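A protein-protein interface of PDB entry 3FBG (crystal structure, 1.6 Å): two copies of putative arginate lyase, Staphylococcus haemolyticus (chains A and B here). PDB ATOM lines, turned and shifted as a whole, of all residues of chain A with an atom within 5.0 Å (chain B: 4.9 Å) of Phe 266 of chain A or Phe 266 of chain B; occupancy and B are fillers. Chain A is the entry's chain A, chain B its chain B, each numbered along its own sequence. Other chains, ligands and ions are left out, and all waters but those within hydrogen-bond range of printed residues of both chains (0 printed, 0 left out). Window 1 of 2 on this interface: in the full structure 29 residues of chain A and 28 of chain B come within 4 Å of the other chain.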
ATOM      1  N   TYR A 231      38.950  -7.450  -6.213  1.00  0.00           N
ATOM      2  CA  TYR A 231      37.530  -7.841  -6.195  1.00  0.00           C
ATOM      3  C   TYR A 231      37.022  -8.292  -7.574  1.00  0.00           C
ATOM      4  O   TYR A 231      36.451  -9.368  -7.726  1.00  0.00           O
ATOM      5  CB  TYR A 231      36.701  -6.643  -5.718  1.00  0.00           C
ATOM      6  CG  TYR A 231      35.216  -6.905  -5.561  1.00  0.00           C
ATOM      7  CD1 TYR A 231      34.744  -7.739  -4.540  1.00  0.00           C
ATOM      8  CD2 TYR A 231      34.273  -6.324  -6.409  1.00  0.00           C
ATOM      9  CE1 TYR A 231      33.373  -7.978  -4.383  1.00  0.00           C
ATOM     10  CE2 TYR A 231      32.917  -6.535  -6.261  1.00  0.00           C
ATOM     11  CZ  TYR A 231      32.447  -7.319  -5.237  1.00  0.00           C
ATOM     12  OH  TYR A 231      31.122  -7.572  -5.092  1.00  0.00           O
ATOM     13  N   HIS A 243      32.847 -19.431  -5.055  1.00  0.00           N
ATOM     14  CA  HIS A 243      32.914 -18.776  -3.743  1.00  0.00           C
ATOM     15  C   HIS A 243      34.196 -18.001  -3.665  1.00  0.00           C
ATOM     16  O   HIS A 243      35.295 -18.515  -3.938  1.00  0.00           O
ATOM     17  CB  HIS A 243      32.885 -19.828  -2.635  1.00  0.00           C
ATOM     18  CG  HIS A 243      32.444 -19.305  -1.295  1.00  0.00           C
ATOM     19  ND1 HIS A 243      31.828 -20.129  -0.370  1.00  0.00           N
ATOM     20  CD2 HIS A 243      32.510 -18.073  -0.719  1.00  0.00           C
ATOM     21  CE1 HIS A 243      31.576 -19.444   0.731  1.00  0.00           C
ATOM     22  NE2 HIS A 243      31.980 -18.192   0.549  1.00  0.00           N
ATOM     23  N   ILE A 244      34.078 -16.701  -3.339  1.00  0.00           N
ATOM     24  CA  ILE A 244      35.223 -15.827  -3.176  1.00  0.00           C
ATOM     25  C   ILE A 244      35.254 -15.269  -1.767  1.00  0.00           C
ATOM     26  O   ILE A 244      34.176 -15.161  -1.148  1.00  0.00           O
ATOM     27  CB  ILE A 244      35.242 -14.673  -4.252  1.00  0.00           C
ATOM     28  CG1 ILE A 244      34.140 -13.636  -4.044  1.00  0.00           C
ATOM     29  CG2 ILE A 244      35.193 -15.238  -5.698  1.00  0.00           C
ATOM     30  CD1 ILE A 244      34.174 -12.341  -5.047  1.00  0.00           C
ATOM     31  N   ALA A 245      36.434 -14.927  -1.275  1.00  0.00           N
ATOM     32  CA  ALA A 245      36.557 -14.474   0.117  1.00  0.00           C
ATOM     33  C   ALA A 245      37.757 -13.598   0.342  1.00  0.00           C
ATOM     34  O   ALA A 245      38.696 -13.617  -0.446  1.00  0.00           O
ATOM     35  CB  ALA A 245      36.603 -15.676   1.068  1.00  0.00           C
ATOM     36  N   THR A 246      37.693 -12.799   1.401  1.00  0.00           N
ATOM     37  CA  THR A 246      38.838 -12.007   1.798  1.00  0.00           C
ATOM     38  C   THR A 246      39.134 -12.213   3.294  1.00  0.00           C
ATOM     39  O   THR A 246      38.245 -12.534   4.056  1.00  0.00           O
ATOM     40  CB  THR A 246      38.605 -10.499   1.473  1.00  0.00           C
ATOM     41  OG1 THR A 246      39.845  -9.780   1.654  1.00  0.00           O
ATOM     42  CG2 THR A 246      37.507  -9.916   2.331  1.00  0.00           C
ATOM     43  N   PHE A 250      38.151  -3.999   3.230  1.00  0.00           N
ATOM     44  CA  PHE A 250      38.036  -3.099   2.062  1.00  0.00           C
ATOM     45  C   PHE A 250      38.258  -1.651   2.488  1.00  0.00           C
ATOM     46  O   PHE A 250      37.820  -1.265   3.567  1.00  0.00           O
ATOM     47  CB  PHE A 250      36.640  -3.202   1.472  1.00  0.00           C
ATOM     48  CG  PHE A 250      36.418  -4.462   0.701  1.00  0.00           C
ATOM     49  CD1 PHE A 250      36.791  -4.527  -0.622  1.00  0.00           C
ATOM     50  CD2 PHE A 250      35.856  -5.575   1.315  1.00  0.00           C
ATOM     51  CE1 PHE A 250      36.605  -5.723  -1.337  1.00  0.00           C
ATOM     52  CE2 PHE A 250      35.632  -6.708   0.601  1.00  0.00           C
ATOM     53  CZ  PHE A 250      36.029  -6.789  -0.708  1.00  0.00           C
ATOM     54  N   LEU A 256      27.765  -5.127  -4.898  1.00  0.00           N
ATOM     55  CA  LEU A 256      27.418  -6.551  -4.673  1.00  0.00           C
ATOM     56  C   LEU A 256      26.648  -7.162  -5.839  1.00  0.00           C
ATOM     57  O   LEU A 256      26.525  -8.404  -5.945  1.00  0.00           O
ATOM     58  CB  LEU A 256      26.652  -6.736  -3.377  1.00  0.00           C
ATOM     59  CG  LEU A 256      27.474  -6.571  -2.103  1.00  0.00           C
ATOM     60  CD1 LEU A 256      26.542  -6.648  -0.924  1.00  0.00           C
ATOM     61  CD2 LEU A 256      28.562  -7.670  -1.988  1.00  0.00           C
ATOM     62  N   LEU A 259      28.304  -9.833  -8.156  1.00  0.00           N
ATOM     63  CA  LEU A 259      28.236 -11.315  -7.795  1.00  0.00           C
ATOM     64  C   LEU A 259      27.087 -11.956  -8.543  1.00  0.00           C
ATOM     65  O   LEU A 259      26.960 -13.160  -8.584  1.00  0.00           O
ATOM     66  CB  LEU A 259      27.995 -11.503  -6.282  1.00  0.00           C
ATOM     67  CG  LEU A 259      29.062 -10.853  -5.382  1.00  0.00           C
ATOM     68  CD1 LEU A 259      28.614 -10.874  -3.916  1.00  0.00           C
ATOM     69  CD2 LEU A 259      30.431 -11.507  -5.565  1.00  0.00           C
ATOM     70  N   LEU A 264      27.267 -15.783  -7.413  1.00  0.00           N
ATOM     71  CA  LEU A 264      28.403 -16.045  -6.507  1.00  0.00           C
ATOM     72  C   LEU A 264      28.168 -15.833  -5.006  1.00  0.00           C
ATOM     73  O   LEU A 264      27.296 -15.059  -4.628  1.00  0.00           O
ATOM     74  CB  LEU A 264      29.611 -15.193  -6.917  1.00  0.00           C
ATOM     75  CG  LEU A 264      30.129 -15.355  -8.341  1.00  0.00           C
ATOM     76  CD1 LEU A 264      31.293 -14.450  -8.604  1.00  0.00           C
ATOM     77  CD2 LEU A 264      30.590 -16.844  -8.558  1.00  0.00           C
ATOM     78  N   SER A 265      29.016 -16.443  -4.173  1.00  0.00           N
ATOM     79  CA  SER A 265      29.061 -16.192  -2.738  1.00  0.00           C
ATOM     80  C   SER A 265      30.336 -15.404  -2.457  1.00  0.00           C
ATOM     81  O   SER A 265      31.371 -15.638  -3.088  1.00  0.00           O
ATOM     82  CB  SER A 265      29.106 -17.544  -1.935  1.00  0.00           C
ATOM     83  OG  SER A 265      27.940 -18.292  -2.257  1.00  0.00           O
ATOM     84  N   PHE A 266      30.249 -14.512  -1.449  1.00  0.00           N
ATOM     85  CA  PHE A 266      31.355 -13.761  -0.971  1.00  0.00           C
ATOM     86  C   PHE A 266      31.342 -13.832   0.538  1.00  0.00           C
ATOM     87  O   PHE A 266      30.290 -13.601   1.185  1.00  0.00           O
ATOM     88  CB  PHE A 266      31.191 -12.233  -1.302  1.00  0.00           C
ATOM     89  CG  PHE A 266      32.277 -11.441  -0.724  1.00  0.00           C
ATOM     90  CD1 PHE A 266      33.454 -11.252  -1.461  1.00  0.00           C
ATOM     91  CD2 PHE A 266      32.173 -10.918   0.576  1.00  0.00           C
ATOM     92  CE1 PHE A 266      34.548 -10.543  -0.899  1.00  0.00           C
ATOM     93  CE2 PHE A 266      33.272 -10.193   1.145  1.00  0.00           C
ATOM     94  CZ  PHE A 266      34.443 -10.052   0.412  1.00  0.00           C
ATOM     95  N   SER A 267      32.506 -14.231   1.092  1.00  0.00           N
ATOM     96  CA  SER A 267      32.682 -14.289   2.552  1.00  0.00           C
ATOM     97  C   SER A 267      33.813 -13.373   3.061  1.00  0.00           C
ATOM     98  O   SER A 267      34.842 -13.193   2.407  1.00  0.00           O
ATOM     99  CB  SER A 267      32.888 -15.776   2.957  1.00  0.00           C
ATOM    100  OG  SER A 267      31.707 -16.497   2.607  1.00  0.00           O
ATOM    101  N   HIS A 268      33.582 -12.745   4.218  1.00  0.00           N
ATOM    102  CA  HIS A 268      34.650 -12.031   4.910  1.00  0.00           C
ATOM    103  C   HIS A 268      35.032 -12.854   6.127  1.00  0.00           C
ATOM    104  O   HIS A 268      34.274 -12.942   7.135  1.00  0.00           O
ATOM    105  CB  HIS A 268      34.053 -10.645   5.322  1.00  0.00           C
ATOM    106  CG  HIS A 268      35.086  -9.618   5.557  1.00  0.00           C
ATOM    107  ND1 HIS A 268      34.907  -8.309   5.150  1.00  0.00           N
ATOM    108  CD2 HIS A 268      36.303  -9.680   6.137  1.00  0.00           C
ATOM    109  CE1 HIS A 268      35.988  -7.614   5.475  1.00  0.00           C
ATOM    110  NE2 HIS A 268      36.848  -8.421   6.076  1.00  0.00           N
ATOM    111  N   TYR B 231      19.916  -4.807   4.293  1.00  0.00           N
ATOM    112  CA  TYR B 231      21.308  -5.317   4.418  1.00  0.00           C
ATOM    113  C   TYR B 231      21.791  -5.331   5.868  1.00  0.00           C
ATOM    114  O   TYR B 231      22.258  -6.369   6.400  1.00  0.00           O
ATOM    115  CB  TYR B 231      22.242  -4.490   3.527  1.00  0.00           C
ATOM    116  CG  TYR B 231      23.691  -4.912   3.485  1.00  0.00           C
ATOM    117  CD1 TYR B 231      24.078  -6.049   2.786  1.00  0.00           C
ATOM    118  CD2 TYR B 231      24.671  -4.152   4.098  1.00  0.00           C
ATOM    119  CE1 TYR B 231      25.417  -6.425   2.712  1.00  0.00           C
ATOM    120  CE2 TYR B 231      26.008  -4.507   4.048  1.00  0.00           C
ATOM    121  CZ  TYR B 231      26.378  -5.641   3.343  1.00  0.00           C
ATOM    122  OH  TYR B 231      27.711  -5.955   3.321  1.00  0.00           O
ATOM    123  N   HIS B 243      24.756 -17.120   7.085  1.00  0.00           N
ATOM    124  CA  HIS B 243      24.758 -16.869   5.658  1.00  0.00           C
ATOM    125  C   HIS B 243      23.539 -16.046   5.290  1.00  0.00           C
ATOM    126  O   HIS B 243      22.399 -16.398   5.648  1.00  0.00           O
ATOM    127  CB  HIS B 243      24.732 -18.248   4.937  1.00  0.00           C
ATOM    128  CG  HIS B 243      25.152 -18.228   3.488  1.00  0.00           C
ATOM    129  ND1 HIS B 243      25.644 -19.356   2.858  1.00  0.00           N
ATOM    130  CD2 HIS B 243      25.130 -17.250   2.540  1.00  0.00           C
ATOM    131  CE1 HIS B 243      25.929 -19.067   1.594  1.00  0.00           C
ATOM    132  NE2 HIS B 243      25.593 -17.802   1.361  1.00  0.00           N
ATOM    133  N   ILE B 244      23.783 -14.945   4.590  1.00  0.00           N
ATOM    134  CA  ILE B 244      22.681 -14.130   4.105  1.00  0.00           C
ATOM    135  C   ILE B 244      22.714 -14.085   2.576  1.00  0.00           C
ATOM    136  O   ILE B 244      23.783 -14.214   1.966  1.00  0.00           O
ATOM    137  CB  ILE B 244      22.756 -12.772   4.750  1.00  0.00           C
ATOM    138  CG1 ILE B 244      23.952 -11.988   4.252  1.00  0.00           C
ATOM    139  CG2 ILE B 244      22.748 -12.891   6.279  1.00  0.00           C
ATOM    140  CD1 ILE B 244      24.208 -10.675   4.980  1.00  0.00           C
ATOM    141  N   ALA B 245      21.540 -13.934   1.941  1.00  0.00           N
ATOM    142  CA  ALA B 245      21.511 -13.947   0.470  1.00  0.00           C
ATOM    143  C   ALA B 245      20.365 -13.077  -0.014  1.00  0.00           C
ATOM    144  O   ALA B 245      19.385 -12.843   0.723  1.00  0.00           O
ATOM    145  CB  ALA B 245      21.319 -15.338  -0.045  1.00  0.00           C
ATOM    146  N   THR B 246      20.460 -12.675  -1.269  1.00  0.00           N
ATOM    147  CA  THR B 246      19.370 -11.941  -1.867  1.00  0.00           C
ATOM    148  C   THR B 246      19.065 -12.491  -3.218  1.00  0.00           C
ATOM    149  O   THR B 246      19.941 -13.118  -3.862  1.00  0.00           O
ATOM    150  CB  THR B 246      19.704 -10.459  -2.003  1.00  0.00           C
ATOM    151  OG1 THR B 246      18.498  -9.764  -2.415  1.00  0.00           O
ATOM    152  CG2 THR B 246      20.755 -10.187  -3.017  1.00  0.00           C
ATOM    153  N   PHE B 250      20.809  -4.800  -5.766  1.00  0.00           N
ATOM    154  CA  PHE B 250      20.912  -3.620  -4.900  1.00  0.00           C
ATOM    155  C   PHE B 250      20.828  -2.391  -5.764  1.00  0.00           C
ATOM    156  O   PHE B 250      21.324  -2.391  -6.888  1.00  0.00           O
ATOM    157  CB  PHE B 250      22.303  -3.607  -4.281  1.00  0.00           C
ATOM    158  CG  PHE B 250      22.467  -4.568  -3.148  1.00  0.00           C
ATOM    159  CD1 PHE B 250      22.170  -4.182  -1.861  1.00  0.00           C
ATOM    160  CD2 PHE B 250      22.973  -5.825  -3.376  1.00  0.00           C
ATOM    161  CE1 PHE B 250      22.324  -5.010  -0.803  1.00  0.00           C
ATOM    162  CE2 PHE B 250      23.126  -6.678  -2.310  1.00  0.00           C
ATOM    163  CZ  PHE B 250      22.812  -6.290  -1.032  1.00  0.00           C
ATOM    164  N   LEU B 256      31.057  -4.187   2.410  1.00  0.00           N
ATOM    165  CA  LEU B 256      31.334  -5.599   2.679  1.00  0.00           C
ATOM    166  C   LEU B 256      32.049  -5.783   4.002  1.00  0.00           C
ATOM    167  O   LEU B 256      32.100  -6.900   4.537  1.00  0.00           O
ATOM    168  CB  LEU B 256      32.163  -6.201   1.543  1.00  0.00           C
ATOM    169  CG  LEU B 256      31.395  -6.526   0.253  1.00  0.00           C
ATOM    170  CD1 LEU B 256      32.297  -7.088  -0.833  1.00  0.00           C
ATOM    171  CD2 LEU B 256      30.143  -7.487   0.457  1.00  0.00           C
ATOM    172  N   LEU B 259      30.261  -7.416   7.012  1.00  0.00           N
ATOM    173  CA  LEU B 259      30.208  -8.896   7.187  1.00  0.00           C
ATOM    174  C   LEU B 259      31.321  -9.377   8.076  1.00  0.00           C
ATOM    175  O   LEU B 259      31.296 -10.542   8.476  1.00  0.00           O
ATOM    176  CB  LEU B 259      30.350  -9.582   5.807  1.00  0.00           C
ATOM    177  CG  LEU B 259      29.316  -9.171   4.754  1.00  0.00           C
ATOM    178  CD1 LEU B 259      29.767  -9.752   3.369  1.00  0.00           C
ATOM    179  CD2 LEU B 259      27.956  -9.699   5.120  1.00  0.00           C
ATOM    180  N   LEU B 264      30.675 -13.415   8.223  1.00  0.00           N
ATOM    181  CA  LEU B 264      29.537 -13.884   7.457  1.00  0.00           C
ATOM    182  C   LEU B 264      29.818 -14.139   5.975  1.00  0.00           C
ATOM    183  O   LEU B 264      30.806 -13.659   5.382  1.00  0.00           O
ATOM    184  CB  LEU B 264      28.384 -12.828   7.516  1.00  0.00           C
ATOM    185  CG  LEU B 264      27.909 -12.520   8.925  1.00  0.00           C
ATOM    186  CD1 LEU B 264      26.853 -11.386   8.853  1.00  0.00           C
ATOM    187  CD2 LEU B 264      27.329 -13.732   9.639  1.00  0.00           C
ATOM    188  N   SER B 265      28.882 -14.881   5.377  1.00  0.00           N
ATOM    189  CA  SER B 265      28.856 -15.088   3.931  1.00  0.00           C
ATOM    190  C   SER B 265      27.626 -14.356   3.346  1.00  0.00           C
ATOM    191  O   SER B 265      26.545 -14.385   3.959  1.00  0.00           O
ATOM    192  CB  SER B 265      28.639 -16.553   3.584  1.00  0.00           C
ATOM    193  OG  SER B 265      29.765 -17.244   4.059  1.00  0.00           O
ATOM    194  N   PHE B 266      27.816 -13.806   2.163  1.00  0.00           N
ATOM    195  CA  PHE B 266      26.730 -13.155   1.420  1.00  0.00           C
ATOM    196  C   PHE B 266      26.642 -13.701   0.029  1.00  0.00           C
ATOM    197  O   PHE B 266      27.663 -13.740  -0.667  1.00  0.00           O
ATOM    198  CB  PHE B 266      26.970 -11.626   1.332  1.00  0.00           C
ATOM    199  CG  PHE B 266      25.884 -10.902   0.568  1.00  0.00           C
ATOM    200  CD1 PHE B 266      24.829 -10.341   1.277  1.00  0.00           C
ATOM    201  CD2 PHE B 266      25.885 -10.881  -0.822  1.00  0.00           C
ATOM    202  CE1 PHE B 266      23.787  -9.724   0.609  1.00  0.00           C
ATOM    203  CE2 PHE B 266      24.803 -10.256  -1.534  1.00  0.00           C
ATOM    204  CZ  PHE B 266      23.770  -9.711  -0.774  1.00  0.00           C
ATOM    205  N   SER B 267      25.453 -14.134  -0.398  1.00  0.00           N
ATOM    206  CA  SER B 267      25.337 -14.665  -1.722  1.00  0.00           C
ATOM    207  C   SER B 267      24.289 -13.907  -2.558  1.00  0.00           C
ATOM    208  O   SER B 267      23.225 -13.505  -2.023  1.00  0.00           O
ATOM    209  CB  SER B 267      24.918 -16.135  -1.674  1.00  0.00           C
ATOM    210  OG  SER B 267      25.987 -16.924  -1.137  1.00  0.00           O
ATOM    211  N   HIS B 268      24.595 -13.762  -3.845  1.00  0.00           N
ATOM    212  CA  HIS B 268      23.624 -13.125  -4.767  1.00  0.00           C
ATOM    213  C   HIS B 268      23.081 -14.259  -5.633  1.00  0.00           C
ATOM    214  O   HIS B 268      23.770 -14.669  -6.575  1.00  0.00           O
ATOM    215  CB  HIS B 268      24.331 -12.105  -5.660  1.00  0.00           C
ATOM    216  CG  HIS B 268      23.389 -11.058  -6.186  1.00  0.00           C
ATOM    217  ND1 HIS B 268      23.674  -9.697  -6.190  1.00  0.00           N
ATOM    218  CD2 HIS B 268      22.126 -11.186  -6.655  1.00  0.00           C
ATOM    219  CE1 HIS B 268      22.634  -9.051  -6.687  1.00  0.00           C
ATOM    220  NE2 HIS B 268      21.667  -9.920  -6.934  1.00  0.00           N
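The backbone carbonyl oxygen (O) of Leu 256 of chain A sits at hydrogen-bond distance from a ring nitrogen (ND1) of His 268 of chain B.
N of His 268 of chain B is in hydrogen-bond range of O of Leu 264 of chain A, 3.1 Å away.
The side-chain hydroxyl of Ser 265 of chain A sits at hydrogen-bond distance from the side-chain hydroxyl of Ser 267 of chain B, 2.6 Å away.
O of Phe 266 of chain A sits at hydrogen-bond distance from N of Phe 266 of chain B, 2.7 Å away.
OG of Ser 267 of chain A sits at hydrogen-bond distance from OG of Ser 265 of chain B, at 2.5 Å.
The backbone carbonyl oxygen (O) of Leu 256 of chain B lies within hydrogen-bond range of a ring nitrogen (ND1) of His 268 of chain A, 3.2 Å away.
The backbone NH (N) of His 268 of chain A sits at hydrogen-bond distance from the backbone carbonyl oxygen (O) of Leu 264 of chain B (3.1 Å).
The backbone NH (N) of Ile 244 of chain A is in hydrogen-bond range of the backbone carbonyl oxygen (O) of Ser 265 of chain A (2.9 Å).
The backbone carbonyl oxygen of Ser 267 of chain A is in hydrogen-bond range of the backbone NH of Thr 246 of chain A, at 3.0 Å.
O of Leu 259 of chain A sits at hydrogen-bond distance from N of Leu 264 of chain A (2.9 Å).
A ring nitrogen (NE2) of His 243 of chain B lies within hydrogen-bond range of the side-chain hydroxyl (OG) of Ser 267 of chain B (2.7 Å).
The backbone carbonyl oxygen (O) of Ser 265 of chain B is in hydrogen-bond range of the backbone NH (N) of Ile 244 of chain B (2.9 Å).
The backbone carbonyl oxygen (O) of Ile 244 of chain B sits at hydrogen-bond distance from the backbone NH (N) of Ser 267 of chain B, at 2.9 Å.
Leu 256 of chain B touches Tyr 231 of chain A (CD1 to CE1, 3.8 Å).
Phe 250 of chain A touches Leu 256 of chain B (CE2 to CB, 3.6 Å).
CD1 of Leu 256 of chain A touches CE1 of Tyr 231 of chain B (3.8 Å).
CB of Leu 256 of chain A touches CE2 of Phe 250 of chain B (3.7 Å).
Leu 256 of chain B touches Leu 256 of chain A (CD2 to CD2, 2.9 Å).
Leu 264 of chain A touches Ser 267 of chain B.
Phe 266 of chain A touches Leu 256 of chain B (CE2 to CD1, 3.8 Å).
Leu 259 of chain B touches Phe 266 of chain A (CD1 to CD2, 3.9 Å).
Ser 265 of chain B touches Phe 266 of chain A.
Ser 267 of chain A touches Leu 264 of chain B (CA to O, 3.5 Å).
Of the printed residues of chain B, Tyr 231 of chain A touches Leu 256 (3.8 Å).
Ile 244 of chain A touches none of the printed residues of chain B.
Of the printed residues of chain B, Leu 259 of chain A touches His 268.
Phe 266 of chain A touches four residues of chain B.
Of the printed residues of chain B, Ser 267 of chain A touches Leu 264 and Ser 265.
Of the printed residues of chain A, Tyr 231 of chain B touches Leu 256.
Of the printed residues of chain A, Phe 266 of chain B touches Ser 265 and Phe 266.
Of the printed residues of chain A, His 268 of chain B touches Leu 256 (3.1 Å), Leu 259 (3.8 Å) and Leu 264 (3.1 Å).
Of the 13 printed residues of chain A, 9 touch a printed residue of chain B.
Hydrophobic or aromatic side chains of chain A that line the printed part of chain B: Tyr 231, Phe 250, Leu 256, Leu 259, Phe 266 and His 268.
Hydrophobic or aromatic side chains of chain B that line the printed part of chain A: Tyr 231, Phe 250, Leu 256, Leu 259, Phe 266 and His 268.
Among the printed residues, 20 pairs touch across the chains.
Among the printed residues, no Asp or Glu carboxylate lies within 4 Å of a Lys or Arg side-chain nitrogen of the other chain.
Leu 256 of chain A touches His 268 of chain B, and with the chains exchanged His 268 of chain A touches Leu 256 of chain B.
Leu 259 of chain A touches His 268 of chain B, and with the chains exchanged His 268 of chain A touches Leu 259 of chain B.
Leu 264 of chain A touches Ser 267 of chain B, and with the chains exchanged Ser 267 of chain A touches Leu 264 of chain B.
Phe 266 of chain B touches its own counterpart, Phe 266 of chain A.
Of the 20 pairs that touch across the chains among the printed residues, 18 have their exchanged pair printed and touching as well.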
